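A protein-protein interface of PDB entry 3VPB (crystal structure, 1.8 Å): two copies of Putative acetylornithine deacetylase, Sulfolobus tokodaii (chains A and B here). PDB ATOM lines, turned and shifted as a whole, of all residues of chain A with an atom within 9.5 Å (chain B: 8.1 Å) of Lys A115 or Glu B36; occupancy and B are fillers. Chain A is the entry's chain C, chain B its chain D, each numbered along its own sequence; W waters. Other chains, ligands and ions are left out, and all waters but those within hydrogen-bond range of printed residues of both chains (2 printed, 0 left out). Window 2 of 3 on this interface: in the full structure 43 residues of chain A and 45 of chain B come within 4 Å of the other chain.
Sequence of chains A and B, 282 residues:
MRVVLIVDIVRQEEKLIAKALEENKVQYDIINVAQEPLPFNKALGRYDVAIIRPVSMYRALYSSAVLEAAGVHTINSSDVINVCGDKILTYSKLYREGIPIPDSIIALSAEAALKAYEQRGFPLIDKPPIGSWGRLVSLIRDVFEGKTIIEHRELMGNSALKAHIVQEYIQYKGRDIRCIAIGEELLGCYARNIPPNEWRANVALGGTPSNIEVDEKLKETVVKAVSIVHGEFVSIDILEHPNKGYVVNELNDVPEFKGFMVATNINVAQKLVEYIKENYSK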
ATOM      1  N   ILE A 105      -8.461 -26.795  10.417  1.00  0.00           N
ATOM      2  CA  ILE A 105      -8.970 -25.962  11.492  1.00  0.00           C
ATOM      3  C   ILE A 105     -10.241 -25.330  10.961  1.00  0.00           C
ATOM      4  O   ILE A 105     -10.247 -24.771   9.857  1.00  0.00           O
ATOM      5  CB  ILE A 105      -7.945 -24.832  11.877  1.00  0.00           C
ATOM      6  CG1 ILE A 105      -6.638 -25.442  12.419  1.00  0.00           C
ATOM      7  CG2 ILE A 105      -8.545 -23.868  12.881  1.00  0.00           C
ATOM      8  CD1 ILE A 105      -5.479 -24.424  12.596  1.00  0.00           C
ATOM      9  N   ILE A 106     -11.318 -25.426  11.728  1.00  0.00           N
ATOM     10  CA  ILE A 106     -12.616 -24.849  11.319  1.00  0.00           C
ATOM     11  C   ILE A 106     -12.815 -23.455  11.951  1.00  0.00           C
ATOM     12  O   ILE A 106     -12.719 -23.286  13.176  1.00  0.00           O
ATOM     13  CB  ILE A 106     -13.769 -25.842  11.690  1.00  0.00           C
ATOM     14  CG1 ILE A 106     -13.564 -27.214  11.002  1.00  0.00           C
ATOM     15  CG2 ILE A 106     -15.150 -25.280  11.422  1.00  0.00           C
ATOM     16  CD1 ILE A 106     -13.192 -27.183   9.506  1.00  0.00           C
ATOM     17  N   ALA A 107     -13.087 -22.460  11.112  1.00  0.00           N
ATOM     18  CA  ALA A 107     -13.327 -21.088  11.579  1.00  0.00           C
ATOM     19  C   ALA A 107     -14.714 -20.612  11.165  1.00  0.00           C
ATOM     20  O   ALA A 107     -15.073 -20.683   9.988  1.00  0.00           O
ATOM     21  CB  ALA A 107     -12.287 -20.152  11.040  1.00  0.00           C
ATOM     22  N   LEU A 108     -15.496 -20.139  12.128  1.00  0.00           N
ATOM     23  CA  LEU A 108     -16.929 -19.915  11.877  1.00  0.00           C
ATOM     24  C   LEU A 108     -17.308 -18.457  11.939  1.00  0.00           C
ATOM     25  O   LEU A 108     -18.489 -18.109  12.071  1.00  0.00           O
ATOM     26  CB  LEU A 108     -17.793 -20.724  12.827  1.00  0.00           C
ATOM     27  CG  LEU A 108     -17.504 -22.214  12.768  1.00  0.00           C
ATOM     28  CD1 LEU A 108     -18.281 -22.887  13.896  1.00  0.00           C
ATOM     29  CD2 LEU A 108     -17.909 -22.771  11.362  1.00  0.00           C
ATOM     30  N   SER A 109     -16.293 -17.613  11.841  1.00  0.00           N
ATOM     31  CA  SER A 109     -16.504 -16.155  11.773  1.00  0.00           C
ATOM     32  C   SER A 109     -15.292 -15.547  11.132  1.00  0.00           C
ATOM     33  O   SER A 109     -14.248 -16.199  10.975  1.00  0.00           O
ATOM     34  CB  SER A 109     -16.715 -15.561  13.167  1.00  0.00           C
ATOM     35  OG  SER A 109     -15.485 -15.482  13.860  1.00  0.00           O
ATOM     36  N   ALA A 110     -15.426 -14.288  10.719  1.00  0.00           N
ATOM     37  CA  ALA A 110     -14.283 -13.558  10.228  1.00  0.00           C
ATOM     38  C   ALA A 110     -13.158 -13.462  11.260  1.00  0.00           C
ATOM     39  O   ALA A 110     -11.976 -13.679  10.933  1.00  0.00           O
ATOM     40  CB  ALA A 110     -14.724 -12.136   9.785  1.00  0.00           C
ATOM     41  N   GLU A 111     -13.529 -13.133  12.497  1.00  0.00           N
ATOM     42  CA  GLU A 111     -12.557 -13.065  13.573  1.00  0.00           C
ATOM     43  C   GLU A 111     -11.838 -14.414  13.770  1.00  0.00           C
ATOM     44  O   GLU A 111     -10.613 -14.457  13.941  1.00  0.00           O
ATOM     45  CB  GLU A 111     -13.206 -12.604  14.882  1.00  0.00           C
ATOM     46  CG  GLU A 111     -12.237 -12.588  16.086  1.00  0.00           C
ATOM     47  CD  GLU A 111     -12.918 -12.237  17.404  1.00  0.00           C
ATOM     48  OE1 GLU A 111     -14.101 -11.837  17.391  1.00  0.00           O
ATOM     49  OE2 GLU A 111     -12.261 -12.361  18.458  1.00  0.00           O
ATOM     50  N   ALA A 112     -12.587 -15.512  13.717  1.00  0.00           N
ATOM     51  CA  ALA A 112     -11.972 -16.815  13.977  1.00  0.00           C
ATOM     52  C   ALA A 112     -11.116 -17.258  12.797  1.00  0.00           C
ATOM     53  O   ALA A 112     -10.129 -17.959  12.972  1.00  0.00           O
ATOM     54  CB  ALA A 112     -13.044 -17.899  14.351  1.00  0.00           C
ATOM     55  N   ALA A 113     -11.477 -16.821  11.596  1.00  0.00           N
ATOM     56  CA  ALA A 113     -10.698 -17.184  10.405  1.00  0.00           C
ATOM     57  C   ALA A 113      -9.305 -16.542  10.455  1.00  0.00           C
ATOM     58  O   ALA A 113      -8.303 -17.176  10.117  1.00  0.00           O
ATOM     59  CB  ALA A 113     -11.449 -16.769   9.126  1.00  0.00           C
ATOM     60  N   LEU A 114      -9.248 -15.284  10.884  1.00  0.00           N
ATOM     61  CA  LEU A 114      -7.967 -14.608  10.989  1.00  0.00           C
ATOM     62  C   LEU A 114      -7.099 -15.281  12.044  1.00  0.00           C
ATOM     63  O   LEU A 114      -5.912 -15.507  11.811  1.00  0.00           O
ATOM     64  CB  LEU A 114      -8.135 -13.087  11.227  1.00  0.00           C
ATOM     65  CG  LEU A 114      -6.858 -12.238  11.200  1.00  0.00           C
ATOM     66  CD1 LEU A 114      -6.113 -12.370   9.876  1.00  0.00           C
ATOM     67  CD2 LEU A 114      -7.214 -10.747  11.458  1.00  0.00           C
ATOM     68  N   LYS A 115      -7.693 -15.646  13.179  1.00  0.00           N
ATOM     69  CA  LYS A 115      -6.978 -16.423  14.207  1.00  0.00           C
ATOM     70  C   LYS A 115      -6.436 -17.763  13.692  1.00  0.00           C
ATOM     71  O   LYS A 115      -5.289 -18.160  13.998  1.00  0.00           O
ATOM     72  CB  LYS A 115      -7.878 -16.641  15.441  1.00  0.00           C
ATOM     73  CG  LYS A 115      -8.071 -15.382  16.234  1.00  0.00           C
ATOM     74  CD  LYS A 115      -8.940 -15.548  17.480  1.00  0.00           C
ATOM     75  CE  LYS A 115      -9.304 -14.158  18.013  1.00  0.00           C
ATOM     76  NZ  LYS A 115     -10.440 -14.243  18.971  1.00  0.00           N
ATOM     77  N   ALA A 116      -7.249 -18.456  12.898  1.00  0.00           N
ATOM     78  CA  ALA A 116      -6.847 -19.729  12.325  1.00  0.00           C
ATOM     79  C   ALA A 116      -5.653 -19.567  11.352  1.00  0.00           C
ATOM     80  O   ALA A 116      -4.752 -20.400  11.350  1.00  0.00           O
ATOM     81  CB  ALA A 116      -8.028 -20.400  11.627  1.00  0.00           C
ATOM     82  N   TYR A 117      -5.659 -18.505  10.533  1.00  0.00           N
ATOM     83  CA  TYR A 117      -4.524 -18.199   9.642  1.00  0.00           C
ATOM     84  C   TYR A 117      -3.244 -17.981  10.449  1.00  0.00           C
ATOM     85  O   TYR A 117      -2.154 -18.421  10.039  1.00  0.00           O
ATOM     86  CB  TYR A 117      -4.769 -16.918   8.824  1.00  0.00           C
ATOM     87  CG  TYR A 117      -5.891 -16.967   7.811  1.00  0.00           C
ATOM     88  CD1 TYR A 117      -6.322 -15.798   7.180  1.00  0.00           C
ATOM     89  CD2 TYR A 117      -6.508 -18.165   7.456  1.00  0.00           C
ATOM     90  CE1 TYR A 117      -7.330 -15.830   6.230  1.00  0.00           C
ATOM     91  CE2 TYR A 117      -7.534 -18.203   6.533  1.00  0.00           C
ATOM     92  CZ  TYR A 117      -7.935 -17.020   5.912  1.00  0.00           C
ATOM     93  OH  TYR A 117      -8.945 -17.012   4.993  1.00  0.00           O
ATOM     94  N   GLU A 118      -3.385 -17.274  11.572  1.00  0.00           N
ATOM     95  CA  GLU A 118      -2.290 -17.016  12.508  1.00  0.00           C
ATOM     96  C   GLU A 118      -1.770 -18.309  13.150  1.00  0.00           C
ATOM     97  O   GLU A 118      -0.565 -18.470  13.309  1.00  0.00           O
ATOM     98  CB  GLU A 118      -2.713 -15.995  13.578  1.00  0.00           C
ATOM     99  CG  GLU A 118      -2.908 -14.560  13.024  1.00  0.00           C
ATOM    100  CD  GLU A 118      -3.719 -13.603  13.938  1.00  0.00           C
ATOM    101  OE1 GLU A 118      -4.416 -14.058  14.882  1.00  0.00           O
ATOM    102  OE2 GLU A 118      -3.675 -12.367  13.684  1.00  0.00           O
ATOM    103  N   GLN A 119      -2.678 -19.227  13.489  1.00  0.00           N
ATOM    104  CA  GLN A 119      -2.319 -20.552  14.031  1.00  0.00           C
ATOM    105  C   GLN A 119      -1.562 -21.446  13.034  1.00  0.00           C
ATOM    106  O   GLN A 119      -0.564 -22.101  13.366  1.00  0.00           O
ATOM    107  CB  GLN A 119      -3.589 -21.281  14.501  1.00  0.00           C
ATOM    108  CG  GLN A 119      -4.123 -20.772  15.826  1.00  0.00           C
ATOM    109  CD  GLN A 119      -5.549 -21.218  16.136  1.00  0.00           C
ATOM    110  OE1 GLN A 119      -6.202 -21.917  15.348  1.00  0.00           O
ATOM    111  NE2 GLN A 119      -6.046 -20.788  17.287  1.00  0.00           N
ATOM    112  N   ARG A 120      -2.061 -21.482  11.811  1.00  0.00           N
ATOM    113  CA  ARG A 120      -1.562 -22.381  10.785  1.00  0.00           C
ATOM    114  C   ARG A 120      -0.287 -21.838  10.122  1.00  0.00           C
ATOM    115  O   ARG A 120       0.649 -22.605   9.875  1.00  0.00           O
ATOM    116  CB  ARG A 120      -2.685 -22.634   9.774  1.00  0.00           C
ATOM    117  CG  ARG A 120      -2.263 -23.157   8.421  1.00  0.00           C
ATOM    118  CD  ARG A 120      -3.048 -24.393   8.073  1.00  0.00           C
ATOM    119  NE  ARG A 120      -2.431 -25.561   8.684  1.00  0.00           N
ATOM    120  CZ  ARG A 120      -3.054 -26.457   9.437  1.00  0.00           C
ATOM    121  NH1 ARG A 120      -4.372 -26.383   9.679  1.00  0.00           N
ATOM    122  NH2 ARG A 120      -2.341 -27.459   9.926  1.00  0.00           N
ATOM    123  N   GLY A 121      -0.246 -20.523   9.900  1.00  0.00           N
ATOM    124  CA  GLY A 121       0.774 -19.855   9.082  1.00  0.00           C
ATOM    125  C   GLY A 121       0.562 -20.041   7.580  1.00  0.00           C
ATOM    126  O   GLY A 121      -0.289 -20.821   7.146  1.00  0.00           O
ATOM    127  N   PHE A 122       1.330 -19.308   6.776  1.00  0.00           N
ATOM    128  CA  PHE A 122       1.194 -19.337   5.310  1.00  0.00           C
ATOM    129  C   PHE A 122       2.313 -20.137   4.627  1.00  0.00           C
ATOM    130  O   PHE A 122       3.389 -20.254   5.190  1.00  0.00           O
ATOM    131  CB  PHE A 122       1.145 -17.898   4.758  1.00  0.00           C
ATOM    132  CG  PHE A 122       0.076 -17.069   5.369  1.00  0.00           C
ATOM    133  CD1 PHE A 122      -1.246 -17.260   5.017  1.00  0.00           C
ATOM    134  CD2 PHE A 122       0.380 -16.132   6.341  1.00  0.00           C
ATOM    135  CE1 PHE A 122      -2.259 -16.507   5.609  1.00  0.00           C
ATOM    136  CE2 PHE A 122      -0.621 -15.388   6.938  1.00  0.00           C
ATOM    137  CZ  PHE A 122      -1.942 -15.566   6.568  1.00  0.00           C
ATOM    138  N   LEU A 124      -1.473 -21.559   3.071  1.00  0.00           N
ATOM    139  CA  LEU A 124      -2.492 -22.483   3.561  1.00  0.00           C
ATOM    140  C   LEU A 124      -3.620 -22.576   2.540  1.00  0.00           C
ATOM    141  O   LEU A 124      -3.716 -21.751   1.631  1.00  0.00           O
ATOM    142  CB  LEU A 124      -3.026 -22.017   4.929  1.00  0.00           C
ATOM    143  CG  LEU A 124      -3.653 -20.608   5.006  1.00  0.00           C
ATOM    144  CD1 LEU A 124      -5.101 -20.631   4.482  1.00  0.00           C
ATOM    145  CD2 LEU A 124      -3.599 -20.145   6.465  1.00  0.00           C
ATOM    146  N   VAL A 143      -1.128 -12.561   4.663  1.00  0.00           N
ATOM    147  CA  VAL A 143      -2.257 -11.978   5.392  1.00  0.00           C
ATOM    148  C   VAL A 143      -3.076 -11.002   4.546  1.00  0.00           C
ATOM    149  O   VAL A 143      -4.263 -10.826   4.798  1.00  0.00           O
ATOM    150  CB  VAL A 143      -1.867 -11.303   6.734  1.00  0.00           C
ATOM    151  CG1 VAL A 143      -2.949 -11.575   7.776  1.00  0.00           C
ATOM    152  CG2 VAL A 143      -0.538 -11.796   7.238  1.00  0.00           C
ATOM    153  N   GLY A 146      -5.373 -13.326   2.721  1.00  0.00           N
ATOM    154  CA  GLY A 146      -6.290 -13.816   3.761  1.00  0.00           C
ATOM    155  C   GLY A 146      -7.378 -12.820   4.124  1.00  0.00           C
ATOM    156  O   GLY A 146      -8.552 -13.147   4.092  1.00  0.00           O
ATOM    157  N   LYS A 147      -6.989 -11.580   4.412  1.00  0.00           N
ATOM    158  CA  LYS A 147      -7.970 -10.571   4.767  1.00  0.00           C
ATOM    159  C   LYS A 147      -9.003 -10.308   3.668  1.00  0.00           C
ATOM    160  O   LYS A 147     -10.195 -10.178   3.961  1.00  0.00           O
ATOM    161  CB  LYS A 147      -7.287  -9.278   5.208  1.00  0.00           C
ATOM    162  CG  LYS A 147      -6.832  -9.322   6.651  1.00  0.00           C
ATOM    163  CD  LYS A 147      -6.128  -8.042   7.066  1.00  0.00           C
ATOM    164  CE  LYS A 147      -5.559  -8.216   8.449  1.00  0.00           C
ATOM    165  NZ  LYS A 147      -5.002  -6.953   8.962  1.00  0.00           N
ATOM    166  N   ILE A 150     -11.481 -13.264   3.498  1.00  0.00           N
ATOM    167  CA  ILE A 150     -12.452 -13.225   4.584  1.00  0.00           C
ATOM    168  C   ILE A 150     -13.556 -12.245   4.266  1.00  0.00           C
ATOM    169  O   ILE A 150     -14.741 -12.520   4.487  1.00  0.00           O
ATOM    170  CB  ILE A 150     -11.740 -12.852   5.927  1.00  0.00           C
ATOM    171  CG1 ILE A 150     -10.929 -14.052   6.460  1.00  0.00           C
ATOM    172  CG2 ILE A 150     -12.715 -12.319   6.957  1.00  0.00           C
ATOM    173  CD1 ILE A 150      -9.925 -13.637   7.560  1.00  0.00           C
ATOM    174  N   HIS A 164     -15.071 -21.459   7.285  1.00  0.00           N
ATOM    175  CA  HIS A 164     -13.763 -21.630   6.653  1.00  0.00           C
ATOM    176  C   HIS A 164     -13.140 -22.920   7.125  1.00  0.00           C
ATOM    177  O   HIS A 164     -12.991 -23.137   8.335  1.00  0.00           O
ATOM    178  CB  HIS A 164     -12.816 -20.495   7.027  1.00  0.00           C
ATOM    179  CG  HIS A 164     -13.318 -19.138   6.651  1.00  0.00           C
ATOM    180  ND1 HIS A 164     -12.694 -18.369   5.700  1.00  0.00           N
ATOM    181  CD2 HIS A 164     -14.350 -18.401   7.126  1.00  0.00           C
ATOM    182  CE1 HIS A 164     -13.336 -17.219   5.580  1.00  0.00           C
ATOM    183  NE2 HIS A 164     -14.351 -17.214   6.428  1.00  0.00           N
ATOM    184  N   VAL A 166      -9.678 -24.303   7.141  1.00  0.00           N
ATOM    185  CA  VAL A 166      -8.290 -23.826   7.032  1.00  0.00           C
ATOM    186  C   VAL A 166      -7.334 -24.994   7.143  1.00  0.00           C
ATOM    187  O   VAL A 166      -7.226 -25.606   8.203  1.00  0.00           O
ATOM    188  CB  VAL A 166      -8.019 -22.745   8.113  1.00  0.00           C
ATOM    189  CG1 VAL A 166      -6.598 -22.212   7.990  1.00  0.00           C
ATOM    190  CG2 VAL A 166      -9.016 -21.606   7.938  1.00  0.00           C
ATOM    191  N   VAL B   7     -21.183 -21.473  22.331  1.00  0.00           N
ATOM    192  CA  VAL B   7     -22.048 -20.329  22.107  1.00  0.00           C
ATOM    193  C   VAL B   7     -21.528 -19.460  20.973  1.00  0.00           C
ATOM    194  O   VAL B   7     -20.355 -19.573  20.576  1.00  0.00           O
ATOM    195  CB  VAL B   7     -22.169 -19.435  23.405  1.00  0.00           C
ATOM    196  CG1 VAL B   7     -22.735 -20.227  24.571  1.00  0.00           C
ATOM    197  CG2 VAL B   7     -20.809 -18.825  23.783  1.00  0.00           C
ATOM    198  N   ILE B  30     -16.827 -22.387  28.638  1.00  0.00           N
ATOM    199  CA  ILE B  30     -17.578 -21.803  27.539  1.00  0.00           C
ATOM    200  C   ILE B  30     -16.589 -21.611  26.386  1.00  0.00           C
ATOM    201  O   ILE B  30     -15.466 -21.110  26.592  1.00  0.00           O
ATOM    202  CB  ILE B  30     -18.235 -20.446  27.937  1.00  0.00           C
ATOM    203  CG1 ILE B  30     -19.319 -20.689  29.012  1.00  0.00           C
ATOM    204  CG2 ILE B  30     -18.799 -19.737  26.701  1.00  0.00           C
ATOM    205  CD1 ILE B  30     -19.994 -19.452  29.612  1.00  0.00           C
ATOM    206  N   ILE B  31     -16.966 -22.063  25.194  1.00  0.00           N
ATOM    207  CA  ILE B  31     -16.236 -21.697  23.988  1.00  0.00           C
ATOM    208  C   ILE B  31     -17.125 -20.865  23.078  1.00  0.00           C
ATOM    209  O   ILE B  31     -18.207 -21.304  22.691  1.00  0.00           O
ATOM    210  CB  ILE B  31     -15.696 -22.922  23.228  1.00  0.00           C
ATOM    211  CG1 ILE B  31     -14.546 -23.551  24.015  1.00  0.00           C
ATOM    212  CG2 ILE B  31     -15.209 -22.500  21.797  1.00  0.00           C
ATOM    213  CD1 ILE B  31     -14.135 -24.942  23.507  1.00  0.00           C
ATOM    214  N   ASN B  32     -16.686 -19.653  22.754  1.00  0.00           N
ATOM    215  CA  ASN B  32     -17.419 -18.852  21.810  1.00  0.00           C
ATOM    216  C   ASN B  32     -16.894 -19.085  20.375  1.00  0.00           C
ATOM    217  O   ASN B  32     -15.794 -18.646  20.013  1.00  0.00           O
ATOM    218  CB  ASN B  32     -17.351 -17.378  22.178  1.00  0.00           C
ATOM    219  CG  ASN B  32     -18.355 -16.564  21.418  1.00  0.00           C
ATOM    220  OD1 ASN B  32     -18.370 -16.589  20.184  1.00  0.00           O
ATOM    221  ND2 ASN B  32     -19.215 -15.836  22.138  1.00  0.00           N
ATOM    222  N   VAL B  33     -17.705 -19.758  19.569  1.00  0.00           N
ATOM    223  CA  VAL B  33     -17.291 -20.131  18.212  1.00  0.00           C
ATOM    224  C   VAL B  33     -17.464 -19.000  17.183  1.00  0.00           C
ATOM    225  O   VAL B  33     -17.140 -19.160  15.996  1.00  0.00           O
ATOM    226  CB  VAL B  33     -17.933 -21.421  17.762  1.00  0.00           C
ATOM    227  CG1 VAL B  33     -17.419 -22.587  18.658  1.00  0.00           C
ATOM    228  CG2 VAL B  33     -19.480 -21.305  17.735  1.00  0.00           C
ATOM    229  N   ALA B  34     -17.957 -17.856  17.635  1.00  0.00           N
ATOM    230  CA  ALA B  34     -17.862 -16.631  16.847  1.00  0.00           C
ATOM    231  C   ALA B  34     -16.492 -15.974  17.079  1.00  0.00           C
ATOM    232  O   ALA B  34     -16.100 -15.062  16.364  1.00  0.00           O
ATOM    233  CB  ALA B  34     -18.988 -15.692  17.190  1.00  0.00           C
ATOM    234  N   GLN B  35     -15.754 -16.443  18.077  1.00  0.00           N
ATOM    235  CA  GLN B  35     -14.451 -15.844  18.353  1.00  0.00           C
ATOM    236  C   GLN B  35     -13.279 -16.776  18.124  1.00  0.00           C
ATOM    237  O   GLN B  35     -12.220 -16.328  17.704  1.00  0.00           O
ATOM    238  CB  GLN B  35     -14.411 -15.271  19.762  1.00  0.00           C
ATOM    239  CG  GLN B  35     -15.436 -14.161  19.971  1.00  0.00           C
ATOM    240  CD  GLN B  35     -15.489 -13.689  21.403  1.00  0.00           C
ATOM    241  OE1 GLN B  35     -15.174 -14.442  22.326  1.00  0.00           O
ATOM    242  NE2 GLN B  35     -15.883 -12.427  21.598  1.00  0.00           N
ATOM    243  N   GLU B  36     -13.465 -18.061  18.392  1.00  0.00           N
ATOM    244  CA  GLU B  36     -12.378 -19.009  18.381  1.00  0.00           C
ATOM    245  C   GLU B  36     -12.542 -20.062  17.279  1.00  0.00           C
ATOM    246  O   GLU B  36     -13.634 -20.644  17.131  1.00  0.00           O
ATOM    247  CB  GLU B  36     -12.317 -19.745  19.729  1.00  0.00           C
ATOM    248  CG  GLU B  36     -12.200 -18.818  20.957  1.00  0.00           C
ATOM    249  CD  GLU B  36     -10.994 -17.868  20.891  1.00  0.00           C
ATOM    250  OE1 GLU B  36     -11.107 -16.758  21.449  1.00  0.00           O
ATOM    251  OE2 GLU B  36      -9.946 -18.206  20.280  1.00  0.00           O
ATOM    252  N   PRO B  37     -11.449 -20.357  16.554  1.00  0.00           N
ATOM    253  CA  PRO B  37     -11.539 -21.499  15.649  1.00  0.00           C
ATOM    254  C   PRO B  37     -11.488 -22.836  16.415  1.00  0.00           C
ATOM    255  O   PRO B  37     -11.063 -22.860  17.574  1.00  0.00           O
ATOM    256  CB  PRO B  37     -10.310 -21.335  14.741  1.00  0.00           C
ATOM    257  CG  PRO B  37      -9.317 -20.491  15.537  1.00  0.00           C
ATOM    258  CD  PRO B  37     -10.081 -19.803  16.653  1.00  0.00           C
ATOM    259  N   LEU B  38     -11.937 -23.921  15.781  1.00  0.00           N
ATOM    260  CA  LEU B  38     -11.903 -25.272  16.390  1.00  0.00           C
ATOM    261  C   LEU B  38     -11.098 -26.211  15.495  1.00  0.00           C
ATOM    262  O   LEU B  38     -11.480 -26.441  14.342  1.00  0.00           O
ATOM    263  CB  LEU B  38     -13.320 -25.839  16.520  1.00  0.00           C
ATOM    264  CG  LEU B  38     -14.377 -25.048  17.310  1.00  0.00           C
ATOM    265  CD1 LEU B  38     -15.736 -25.755  17.266  1.00  0.00           C
ATOM    266  CD2 LEU B  38     -13.917 -24.844  18.740  1.00  0.00           C
ATOM    267  N   PRO B  39     -10.000 -26.780  16.015  1.00  0.00           N
ATOM    268  CA  PRO B  39      -9.213 -27.672  15.175  1.00  0.00           C
ATOM    269  C   PRO B  39      -9.798 -29.090  15.199  1.00  0.00           C
ATOM    270  O   PRO B  39     -10.469 -29.453  16.173  1.00  0.00           O
ATOM    271  CB  PRO B  39      -7.857 -27.663  15.862  1.00  0.00           C
ATOM    272  CG  PRO B  39      -8.187 -27.492  17.321  1.00  0.00           C
ATOM    273  CD  PRO B  39      -9.438 -26.655  17.385  1.00  0.00           C
ATOM    274  N   SER B  63     -19.860 -26.807  14.833  1.00  0.00           N
ATOM    275  CA  SER B  63     -19.240 -26.945  16.134  1.00  0.00           C
ATOM    276  C   SER B  63     -19.525 -28.360  16.696  1.00  0.00           C
ATOM    277  O   SER B  63     -18.633 -29.014  17.216  1.00  0.00           O
ATOM    278  CB  SER B  63     -19.652 -25.814  17.104  1.00  0.00           C
ATOM    279  OG  SER B  63     -21.018 -25.880  17.443  1.00  0.00           O
HETATM  280  O   HOH W   1      -8.606 -22.062  18.696  1.00  0.00           O
HETATM  281  O   HOH W   2     -15.036 -20.684  14.841  1.00  0.00           O
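No position is printed for both chains.
The backbone NH (N) of Leu B38 sits at hydrogen-bond distance from the backbone carbonyl oxygen (O) of Ile A106 (2.8 Å). The side-chain hydroxyl (OG) of Ser A109 is in hydrogen-bond range of the backbone carbonyl oxygen (O) of Ala B34, at 2.6 Å. NZ of Lys A115 sits at hydrogen-bond distance from O of Gln B35 (3.0 Å). The side-chain amino group (NZ) of Lys A115 lies within salt-bridge range of the side-chain carboxylate (OE1) of Glu B36, 3.6 Å away.
N of Ile A105 is in hydrogen-bond range of O of Val A166 (2.8 Å). N of Glu A111 sits close to OG of Ser A109, 3.3 Å away. OG of Ser A109 sits at hydrogen-bond distance from N of Ala A112 (2.9 Å). The side-chain amino group (NZ) of Lys A115 is in salt-bridge range of the side-chain carboxylate (OE2) of Glu A111, at 2.7 Å. The side-chain amide oxygen (OD1) of Asn B32 sits at hydrogen-bond distance from the backbone NH (N) of Ala B34. N of Gln B35 lies within hydrogen-bond range of OD1 of Asn B32, at 3.4 Å.
Lys A115 touches just these residues of chain B: Gln B35 and Glu B36. Of chain B, only Pro B37 (3.9 Å) comes within 4 Å of Ala A116. Pro B37 touches five residues of chain A. Of the printed residues of chain B, Gln A119 touches Pro B37. Printed residues of chain A within 4 Å of Ala B34: Ser A109 (2.6 Å) and Glu A111 (3.9 Å). Printed residues of chain B within 4 Å of Ser A109: Ala B34. Val A166 touches none of the printed residues of chain B.
Water W2 lies within hydrogen-bond range of O of Glu B36 (2.7 Å), N of Leu A108 (2.8 Å) and O of Val B33 (2.8 Å). Water W1 bridges O of Pro B37 and NE2 of Gln A119.
Ile A105 touches Leu B38. Ile A106 touches Pro B37. Leu A108 touches Val B33 (CB to O, 3.6 Å). Glu A111 touches Ala B34 (OE1 to O, 3.9 Å). Gln B35 touches Glu A111. O of Gln B35 touches CA of Ala A112, at 3.8 Å. Ala A112 touches Glu B36 (CB to C, 3.7 Å). Ala A112 touches Pro B37. Ala A116 touches Pro B37 (N to CG, 3.9 Å). Pro B37 touches Gln A119 (CG to OE1, 3.4 Å).
Of the 25 printed residues of chain A, 9 touch a printed residue of chain B. Printed residues of chain B that touch a printed residue of chain A: Val B33, Ala B34, Gln B35, Glu B36, Pro B37 and Leu B38. Hydrophobic or aromatic side chains of chain B within 4 Å of the printed part of chain A: Pro B37.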
